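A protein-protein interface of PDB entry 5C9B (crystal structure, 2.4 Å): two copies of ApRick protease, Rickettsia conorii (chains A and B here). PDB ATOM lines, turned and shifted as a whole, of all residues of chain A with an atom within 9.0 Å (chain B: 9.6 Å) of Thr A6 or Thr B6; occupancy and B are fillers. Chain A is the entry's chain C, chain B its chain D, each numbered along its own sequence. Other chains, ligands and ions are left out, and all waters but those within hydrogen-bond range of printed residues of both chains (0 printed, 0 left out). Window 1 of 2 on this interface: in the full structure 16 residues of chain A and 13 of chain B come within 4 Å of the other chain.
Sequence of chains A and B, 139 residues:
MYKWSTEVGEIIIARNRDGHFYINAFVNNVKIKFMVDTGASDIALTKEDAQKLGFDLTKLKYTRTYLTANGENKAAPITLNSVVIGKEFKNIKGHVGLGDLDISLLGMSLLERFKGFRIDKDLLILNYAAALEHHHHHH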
ATOM      1  N   LYS A   3      15.674 -16.532  -2.900  1.00  0.00           N
ATOM      2  CA  LYS A   3      16.517 -17.676  -3.067  1.00  0.00           C
ATOM      3  C   LYS A   3      15.760 -18.959  -2.835  1.00  0.00           C
ATOM      4  O   LYS A   3      15.119 -19.113  -1.817  1.00  0.00           O
ATOM      5  CB  LYS A   3      17.643 -17.600  -2.071  1.00  0.00           C
ATOM      6  CG  LYS A   3      18.620 -18.716  -2.303  1.00  0.00           C
ATOM      7  CD  LYS A   3      19.872 -18.498  -1.487  1.00  0.00           C
ATOM      8  CE  LYS A   3      20.542 -19.830  -1.231  1.00  0.00           C
ATOM      9  NZ  LYS A   3      20.803 -19.964   0.218  1.00  0.00           N
ATOM     10  N   TRP A   4      15.877 -19.886  -3.772  1.00  0.00           N
ATOM     11  CA  TRP A   4      15.150 -21.140  -3.705  1.00  0.00           C
ATOM     12  C   TRP A   4      16.080 -22.248  -4.216  1.00  0.00           C
ATOM     13  O   TRP A   4      17.033 -21.992  -4.950  1.00  0.00           O
ATOM     14  CB  TRP A   4      13.894 -20.956  -4.575  1.00  0.00           C
ATOM     15  CG  TRP A   4      13.166 -22.151  -4.971  1.00  0.00           C
ATOM     16  CD1 TRP A   4      12.099 -22.710  -4.336  1.00  0.00           C
ATOM     17  CD2 TRP A   4      13.380 -22.924  -6.163  1.00  0.00           C
ATOM     18  NE1 TRP A   4      11.643 -23.809  -5.049  1.00  0.00           N
ATOM     19  CE2 TRP A   4      12.411 -23.955  -6.175  1.00  0.00           C
ATOM     20  CE3 TRP A   4      14.292 -22.842  -7.227  1.00  0.00           C
ATOM     21  CZ2 TRP A   4      12.340 -24.904  -7.204  1.00  0.00           C
ATOM     22  CZ3 TRP A   4      14.217 -23.790  -8.261  1.00  0.00           C
ATOM     23  CH2 TRP A   4      13.248 -24.801  -8.237  1.00  0.00           C
ATOM     24  N   SER A   5      15.754 -23.478  -3.906  1.00  0.00           N
ATOM     25  CA  SER A   5      16.495 -24.619  -4.443  1.00  0.00           C
ATOM     26  C   SER A   5      15.715 -25.923  -4.315  1.00  0.00           C
ATOM     27  O   SER A   5      14.826 -26.007  -3.486  1.00  0.00           O
ATOM     28  CB  SER A   5      17.760 -24.792  -3.639  1.00  0.00           C
ATOM     29  OG  SER A   5      17.379 -25.025  -2.284  1.00  0.00           O
ATOM     30  N   THR A   6      16.045 -26.936  -5.121  1.00  0.00           N
ATOM     31  CA  THR A   6      15.498 -28.286  -4.919  1.00  0.00           C
ATOM     32  C   THR A   6      16.460 -29.361  -5.399  1.00  0.00           C
ATOM     33  O   THR A   6      17.486 -29.074  -5.993  1.00  0.00           O
ATOM     34  CB  THR A   6      14.215 -28.534  -5.707  1.00  0.00           C
ATOM     35  OG1 THR A   6      14.481 -28.243  -7.090  1.00  0.00           O
ATOM     36  CG2 THR A   6      13.036 -27.712  -5.158  1.00  0.00           C
ATOM     37  N   GLU A   7      16.092 -30.607  -5.131  1.00  0.00           N
ATOM     38  CA  GLU A   7      16.832 -31.743  -5.582  1.00  0.00           C
ATOM     39  C   GLU A   7      16.232 -32.106  -6.931  1.00  0.00           C
ATOM     40  O   GLU A   7      15.041 -32.129  -7.108  1.00  0.00           O
ATOM     41  CB  GLU A   7      16.687 -32.881  -4.572  1.00  0.00           C
ATOM     42  CG  GLU A   7      17.418 -34.175  -4.904  1.00  0.00           C
ATOM     43  CD  GLU A   7      16.482 -35.381  -4.976  1.00  0.00           C
ATOM     44  OE1 GLU A   7      16.889 -36.476  -4.535  1.00  0.00           O
ATOM     45  OE2 GLU A   7      15.341 -35.241  -5.483  1.00  0.00           O
ATOM     46  N   VAL A   8      17.098 -32.366  -7.889  1.00  0.00           N
ATOM     47  CA  VAL A   8      16.711 -32.734  -9.225  1.00  0.00           C
ATOM     48  C   VAL A   8      17.405 -34.058  -9.454  1.00  0.00           C
ATOM     49  O   VAL A   8      18.461 -34.326  -8.869  1.00  0.00           O
ATOM     50  CB  VAL A   8      17.189 -31.676 -10.223  1.00  0.00           C
ATOM     51  CG1 VAL A   8      17.585 -32.276 -11.555  1.00  0.00           C
ATOM     52  CG2 VAL A   8      16.075 -30.648 -10.413  1.00  0.00           C
ATOM     53  N   GLY A   9      16.801 -34.897 -10.279  1.00  0.00           N
ATOM     54  CA  GLY A   9      17.374 -36.192 -10.545  1.00  0.00           C
ATOM     55  C   GLY A   9      16.996 -36.847 -11.855  1.00  0.00           C
ATOM     56  O   GLY A   9      16.006 -36.468 -12.540  1.00  0.00           O
ATOM     57  N   GLU A  10      17.809 -37.845 -12.185  1.00  0.00           N
ATOM     58  CA  GLU A  10      17.660 -38.650 -13.384  1.00  0.00           C
ATOM     59  C   GLU A  10      17.899 -40.102 -13.027  1.00  0.00           C
ATOM     60  O   GLU A  10      18.905 -40.440 -12.392  1.00  0.00           O
ATOM     61  CB  GLU A  10      18.681 -38.262 -14.455  1.00  0.00           C
ATOM     62  CG  GLU A  10      18.407 -38.913 -15.814  1.00  0.00           C
ATOM     63  CD  GLU A  10      19.104 -38.229 -17.007  1.00  0.00           C
ATOM     64  OE1 GLU A  10      20.341 -38.236 -17.062  1.00  0.00           O
ATOM     65  OE2 GLU A  10      18.417 -37.727 -17.922  1.00  0.00           O
ATOM     66  N   LYS A 115       8.134 -35.594 -14.227  1.00  0.00           N
ATOM     67  CA  LYS A 115       8.555 -34.449 -14.973  1.00  0.00           C
ATOM     68  C   LYS A 115       9.012 -34.898 -16.320  1.00  0.00           C
ATOM     69  O   LYS A 115       8.509 -34.442 -17.331  1.00  0.00           O
ATOM     70  CB  LYS A 115       9.695 -33.801 -14.204  1.00  0.00           C
ATOM     71  CG  LYS A 115      10.484 -32.778 -14.973  1.00  0.00           C
ATOM     72  CD  LYS A 115      11.747 -32.395 -14.211  1.00  0.00           C
ATOM     73  CE  LYS A 115      12.815 -31.902 -15.186  1.00  0.00           C
ATOM     74  NZ  LYS A 115      14.076 -31.603 -14.462  1.00  0.00           N
ATOM     75  N   TYR A 128      13.057 -36.162 -12.553  1.00  0.00           N
ATOM     76  CA  TYR A 128      12.200 -35.782 -11.459  1.00  0.00           C
ATOM     77  C   TYR A 128      12.812 -34.652 -10.652  1.00  0.00           C
ATOM     78  O   TYR A 128      14.025 -34.425 -10.714  1.00  0.00           O
ATOM     79  CB  TYR A 128      12.004 -36.965 -10.503  1.00  0.00           C
ATOM     80  CG  TYR A 128      13.233 -37.434  -9.774  1.00  0.00           C
ATOM     81  CD1 TYR A 128      13.620 -36.872  -8.550  1.00  0.00           C
ATOM     82  CD2 TYR A 128      13.998 -38.449 -10.295  1.00  0.00           C
ATOM     83  CE1 TYR A 128      14.764 -37.310  -7.888  1.00  0.00           C
ATOM     84  CE2 TYR A 128      15.131 -38.906  -9.639  1.00  0.00           C
ATOM     85  CZ  TYR A 128      15.520 -38.346  -8.451  1.00  0.00           C
ATOM     86  OH  TYR A 128      16.656 -38.869  -7.846  1.00  0.00           O
ATOM     87  N   ALA A 129      11.958 -33.988  -9.874  1.00  0.00           N
ATOM     88  CA  ALA A 129      12.372 -32.950  -8.929  1.00  0.00           C
ATOM     89  C   ALA A 129      11.652 -33.051  -7.545  1.00  0.00           C
ATOM     90  O   ALA A 129      10.493 -33.371  -7.465  1.00  0.00           O
ATOM     91  CB  ALA A 129      12.155 -31.596  -9.569  1.00  0.00           C
ATOM     92  N   ALA A 130      12.377 -32.807  -6.462  1.00  0.00           N
ATOM     93  CA  ALA A 130      11.855 -32.896  -5.099  1.00  0.00           C
ATOM     94  C   ALA A 130      11.748 -31.513  -4.374  1.00  0.00           C
ATOM     95  O   ALA A 130      11.224 -30.550  -4.951  1.00  0.00           O
ATOM     96  CB  ALA A 130      12.721 -33.876  -4.318  1.00  0.00           C
ATOM     97  N   ALA A 131      12.201 -31.427  -3.116  1.00  0.00           N
ATOM     98  CA  ALA A 131      12.212 -30.164  -2.358  1.00  0.00           C
ATOM     99  C   ALA A 131      13.171 -30.237  -1.167  1.00  0.00           C
ATOM    100  O   ALA A 131      14.140 -29.485  -1.100  1.00  0.00           O
ATOM    101  CB  ALA A 131      10.810 -29.811  -1.888  1.00  0.00           C
ATOM    102  N   LYS B   3      21.652 -43.722 -11.596  1.00  0.00           N
ATOM    103  CA  LYS B   3      20.856 -42.838 -10.788  1.00  0.00           C
ATOM    104  C   LYS B   3      21.716 -41.645 -10.486  1.00  0.00           C
ATOM    105  O   LYS B   3      22.841 -41.805 -10.083  1.00  0.00           O
ATOM    106  CB  LYS B   3      20.442 -43.485  -9.469  1.00  0.00           C
ATOM    107  CG  LYS B   3      19.636 -42.511  -8.604  1.00  0.00           C
ATOM    108  CD  LYS B   3      18.754 -43.161  -7.544  1.00  0.00           C
ATOM    109  CE  LYS B   3      17.992 -42.091  -6.761  1.00  0.00           C
ATOM    110  NZ  LYS B   3      17.469 -42.580  -5.449  1.00  0.00           N
ATOM    111  N   TRP B   4      21.184 -40.441 -10.652  1.00  0.00           N
ATOM    112  CA  TRP B   4      21.994 -39.267 -10.514  1.00  0.00           C
ATOM    113  C   TRP B   4      21.144 -38.205  -9.808  1.00  0.00           C
ATOM    114  O   TRP B   4      19.963 -38.085 -10.103  1.00  0.00           O
ATOM    115  CB  TRP B   4      22.519 -38.849 -11.957  1.00  0.00           C
ATOM    116  CG  TRP B   4      23.197 -37.505 -11.987  1.00  0.00           C
ATOM    117  CD1 TRP B   4      24.484 -37.223 -11.607  1.00  0.00           C
ATOM    118  CD2 TRP B   4      22.597 -36.237 -12.319  1.00  0.00           C
ATOM    119  NE1 TRP B   4      24.724 -35.864 -11.704  1.00  0.00           N
ATOM    120  CE2 TRP B   4      23.580 -35.241 -12.134  1.00  0.00           C
ATOM    121  CE3 TRP B   4      21.315 -35.843 -12.736  1.00  0.00           C
ATOM    122  CZ2 TRP B   4      23.327 -33.884 -12.382  1.00  0.00           C
ATOM    123  CZ3 TRP B   4      21.070 -34.489 -12.992  1.00  0.00           C
ATOM    124  CH2 TRP B   4      22.068 -33.534 -12.808  1.00  0.00           C
ATOM    125  N   SER B   5      21.713 -37.429  -8.880  1.00  0.00           N
ATOM    126  CA  SER B   5      21.010 -36.204  -8.439  1.00  0.00           C
ATOM    127  C   SER B   5      21.840 -34.955  -8.018  1.00  0.00           C
ATOM    128  O   SER B   5      23.029 -35.031  -7.797  1.00  0.00           O
ATOM    129  CB  SER B   5      20.113 -36.596  -7.324  1.00  0.00           C
ATOM    130  OG  SER B   5      20.957 -37.240  -6.431  1.00  0.00           O
ATOM    131  N   THR B   6      21.194 -33.800  -7.914  1.00  0.00           N
ATOM    132  CA  THR B   6      21.907 -32.550  -7.591  1.00  0.00           C
ATOM    133  C   THR B   6      20.980 -31.477  -7.065  1.00  0.00           C
ATOM    134  O   THR B   6      19.787 -31.555  -7.249  1.00  0.00           O
ATOM    135  CB  THR B   6      22.595 -31.943  -8.836  1.00  0.00           C
ATOM    136  OG1 THR B   6      21.742 -32.090  -9.973  1.00  0.00           O
ATOM    137  CG2 THR B   6      23.941 -32.627  -9.130  1.00  0.00           C
ATOM    138  N   GLU B   7      21.553 -30.483  -6.401  1.00  0.00           N
ATOM    139  CA  GLU B   7      20.817 -29.320  -5.895  1.00  0.00           C
ATOM    140  C   GLU B   7      20.735 -28.295  -7.041  1.00  0.00           C
ATOM    141  O   GLU B   7      21.746 -27.930  -7.612  1.00  0.00           O
ATOM    142  CB  GLU B   7      21.546 -28.724  -4.698  1.00  0.00           C
ATOM    143  CG  GLU B   7      20.805 -27.624  -3.937  1.00  0.00           C
ATOM    144  CD  GLU B   7      21.715 -26.467  -3.506  1.00  0.00           C
ATOM    145  OE1 GLU B   7      22.925 -26.703  -3.283  1.00  0.00           O
ATOM    146  OE2 GLU B   7      21.225 -25.311  -3.395  1.00  0.00           O
ATOM    147  N   VAL B   8      19.534 -27.877  -7.412  1.00  0.00           N
ATOM    148  CA  VAL B   8      19.375 -26.803  -8.379  1.00  0.00           C
ATOM    149  C   VAL B   8      18.868 -25.598  -7.640  1.00  0.00           C
ATOM    150  O   VAL B   8      17.963 -25.726  -6.862  1.00  0.00           O
ATOM    151  CB  VAL B   8      18.367 -27.173  -9.456  1.00  0.00           C
ATOM    152  CG1 VAL B   8      17.753 -25.936 -10.067  1.00  0.00           C
ATOM    153  CG2 VAL B   8      19.069 -28.005 -10.513  1.00  0.00           C
ATOM    154  N   GLY B   9      19.431 -24.433  -7.914  1.00  0.00           N
ATOM    155  CA  GLY B   9      19.039 -23.223  -7.211  1.00  0.00           C
ATOM    156  C   GLY B   9      18.764 -22.019  -8.072  1.00  0.00           C
ATOM    157  O   GLY B   9      19.194 -21.927  -9.229  1.00  0.00           O
ATOM    158  N   GLU B  10      18.031 -21.085  -7.491  1.00  0.00           N
ATOM    159  CA  GLU B  10      17.771 -19.820  -8.156  1.00  0.00           C
ATOM    160  C   GLU B  10      17.828 -18.682  -7.146  1.00  0.00           C
ATOM    161  O   GLU B  10      17.259 -18.759  -6.058  1.00  0.00           O
ATOM    162  CB  GLU B  10      16.433 -19.852  -8.873  1.00  0.00           C
ATOM    163  CG  GLU B  10      16.298 -18.723  -9.880  1.00  0.00           C
ATOM    164  CD  GLU B  10      15.143 -18.854 -10.878  1.00  0.00           C
ATOM    165  OE1 GLU B  10      14.078 -19.452 -10.607  1.00  0.00           O
ATOM    166  OE2 GLU B  10      15.307 -18.325 -11.984  1.00  0.00           O
ATOM    167  N   LYS B  87      26.299 -21.374  -4.739  1.00  0.00           N
ATOM    168  CA  LYS B  87      27.205 -22.524  -4.663  1.00  0.00           C
ATOM    169  C   LYS B  87      28.623 -21.998  -4.514  1.00  0.00           C
ATOM    170  O   LYS B  87      28.820 -20.790  -4.538  1.00  0.00           O
ATOM    171  CB  LYS B  87      27.051 -23.432  -5.907  1.00  0.00           C
ATOM    172  CG  LYS B  87      27.642 -22.925  -7.227  1.00  0.00           C
ATOM    173  CD  LYS B  87      27.523 -24.009  -8.311  1.00  0.00           C
ATOM    174  CE  LYS B  87      28.718 -24.103  -9.261  1.00  0.00           C
ATOM    175  NZ  LYS B  87      28.312 -24.266 -10.693  1.00  0.00           N
ATOM    176  N   LYS B 115      25.212 -21.593 -14.437  1.00  0.00           N
ATOM    177  CA  LYS B 115      24.266 -22.189 -15.355  1.00  0.00           C
ATOM    178  C   LYS B 115      23.394 -21.133 -16.013  1.00  0.00           C
ATOM    179  O   LYS B 115      23.053 -21.239 -17.194  1.00  0.00           O
ATOM    180  CB  LYS B 115      23.423 -23.197 -14.582  1.00  0.00           C
ATOM    181  CG  LYS B 115      22.351 -23.937 -15.348  1.00  0.00           C
ATOM    182  CD  LYS B 115      21.591 -24.901 -14.418  1.00  0.00           C
ATOM    183  CE  LYS B 115      20.163 -25.164 -14.913  1.00  0.00           C
ATOM    184  NZ  LYS B 115      19.157 -25.119 -13.815  1.00  0.00           N
ATOM    185  N   TYR B 128      21.916 -21.858 -10.637  1.00  0.00           N
ATOM    186  CA  TYR B 128      23.117 -22.631 -10.424  1.00  0.00           C
ATOM    187  C   TYR B 128      22.777 -24.082 -10.145  1.00  0.00           C
ATOM    188  O   TYR B 128      21.621 -24.418  -9.837  1.00  0.00           O
ATOM    189  CB  TYR B 128      23.914 -22.035  -9.263  1.00  0.00           C
ATOM    190  CG  TYR B 128      23.115 -21.922  -7.983  1.00  0.00           C
ATOM    191  CD1 TYR B 128      22.994 -23.011  -7.114  1.00  0.00           C
ATOM    192  CD2 TYR B 128      22.472 -20.742  -7.639  1.00  0.00           C
ATOM    193  CE1 TYR B 128      22.263 -22.926  -5.936  1.00  0.00           C
ATOM    194  CE2 TYR B 128      21.733 -20.654  -6.458  1.00  0.00           C
ATOM    195  CZ  TYR B 128      21.633 -21.744  -5.607  1.00  0.00           C
ATOM    196  OH  TYR B 128      20.897 -21.671  -4.432  1.00  0.00           O
ATOM    197  N   ALA B 129      23.791 -24.938 -10.271  1.00  0.00           N
ATOM    198  CA  ALA B 129      23.644 -26.339  -9.915  1.00  0.00           C
ATOM    199  C   ALA B 129      24.903 -26.817  -9.248  1.00  0.00           C
ATOM    200  O   ALA B 129      25.983 -26.641  -9.784  1.00  0.00           O
ATOM    201  CB  ALA B 129      23.328 -27.202 -11.126  1.00  0.00           C
ATOM    202  N   ALA B 130      24.714 -27.389  -8.065  1.00  0.00           N
ATOM    203  CA  ALA B 130      25.714 -28.081  -7.270  1.00  0.00           C
ATOM    204  C   ALA B 130      25.379 -29.580  -7.259  1.00  0.00           C
ATOM    205  O   ALA B 130      24.532 -30.022  -8.027  1.00  0.00           O
ATOM    206  CB  ALA B 130      25.688 -27.527  -5.860  1.00  0.00           C
ATOM    207  N   ALA B 131      26.066 -30.354  -6.412  1.00  0.00           N
ATOM    208  CA  ALA B 131      25.768 -31.781  -6.192  1.00  0.00           C
ATOM    209  C   ALA B 131      25.879 -32.106  -4.718  1.00  0.00           C
ATOM    210  O   ALA B 131      24.849 -32.174  -4.039  1.00  0.00           O
ATOM    211  CB  ALA B 131      26.692 -32.670  -6.999  1.00  0.00           C
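Trp A4 touches Gly B9, and with the chains exchanged Gly A9 touches Trp B4.
Trp A4 touches Glu B10, and with the chains exchanged Glu A10 touches Trp B4.
Thr A6 touches Val B8, and with the chains exchanged Val A8 touches Thr B6.
Val A8 touches its own counterpart, Val B8.
13 positions are printed for both chains.
Of the 18 pairs that touch across the chains among the printed residues, 16 have their exchanged pair printed and touching as well.
Printed residues of chain B within 4 Å of Ser A5: Glu B7 (3.5 Å) and Val B8 (3.0 Å).
Thr A6 touches just these residues of chain B: Thr B6 (3.6 Å), Glu B7 (3.3 Å) and Val B8 (2.8 Å).
Printed residues of chain A within 4 Å of Lys B3: Glu A10 (3.5 Å) and Tyr A128 (3.7 Å).
Of chain A, only Val A8 (3.2 Å) comes within 4 Å of Ser B5.
Of chain A, only Thr A6, Glu A7 and Val A8 come within 4 Å of Thr B6.
Printed residues of chain A within 4 Å of Gly B9: Trp A4.
The nearest residue of chain B that does not touch Thr A6 is Gly B9 (5.1 Å).
The nearest printed residue of chain B that does not touch Lys A3 is Glu B7 (5.9 Å).
Among the printed residues, pairs that only touch across the chains: Lys A3 with Glu B10 (3.3 Å), Lys A3 with Tyr B128 (3.7 Å), Trp A4 with Gly B9 (3.3 Å), Trp A4 with Tyr B128 (3.9 Å), Ser A5 with Glu B7 (3.5 Å), Ser A5 with Val B8 (3.0 Å), Thr A6 with Thr B6 (3.6 Å), Thr A6 with Glu B7 (3.3 Å), Glu A7 with Thr B6 (3.4 Å), Val A8 with Ser B5 (3.2 Å), Val A8 with Val B8 (3.99 Å), Gly A9 with Trp B4 (3.2 Å), Glu A10 with Lys B3 (3.5 Å) and Tyr A128 with Lys B3 (3.7 Å).
O of Trp A4 sits at hydrogen-bond distance from N of Glu B10 (2.9 Å).
O of Thr A6 is in hydrogen-bond range of N of Val B8, at 2.8 Å.
The backbone NH (N) of Val A8 is in hydrogen-bond range of the backbone carbonyl oxygen (O) of Thr B6, 2.9 Å away.
The backbone carbonyl oxygen (O) of Glu A10 sits at hydrogen-bond distance from the backbone NH (N) of Trp B4, 2.9 Å away.
N of Ala A130 is in hydrogen-bond range of O of Glu A7 (2.8 Å).
The backbone NH (N) of Gly A9 is in hydrogen-bond range of the backbone carbonyl oxygen (O) of Tyr A128 (2.8 Å).
O of Glu B7 is in hydrogen-bond range of N of Ala B130.
O of Tyr B128 lies within hydrogen-bond range of N of Gly B9, 2.9 Å away.
Of the 13 printed residues of chain A, 9 touch a printed residue of chain B.
Of the 14 printed residues of chain B, 9 touch a printed residue of chain A.
Hydrophobic or aromatic side chains of chain B within 4 Å of the printed part of chain A: Trp B4, Val B8 and Tyr B128.
Among the printed residues, 18 pairs touch across the chains.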
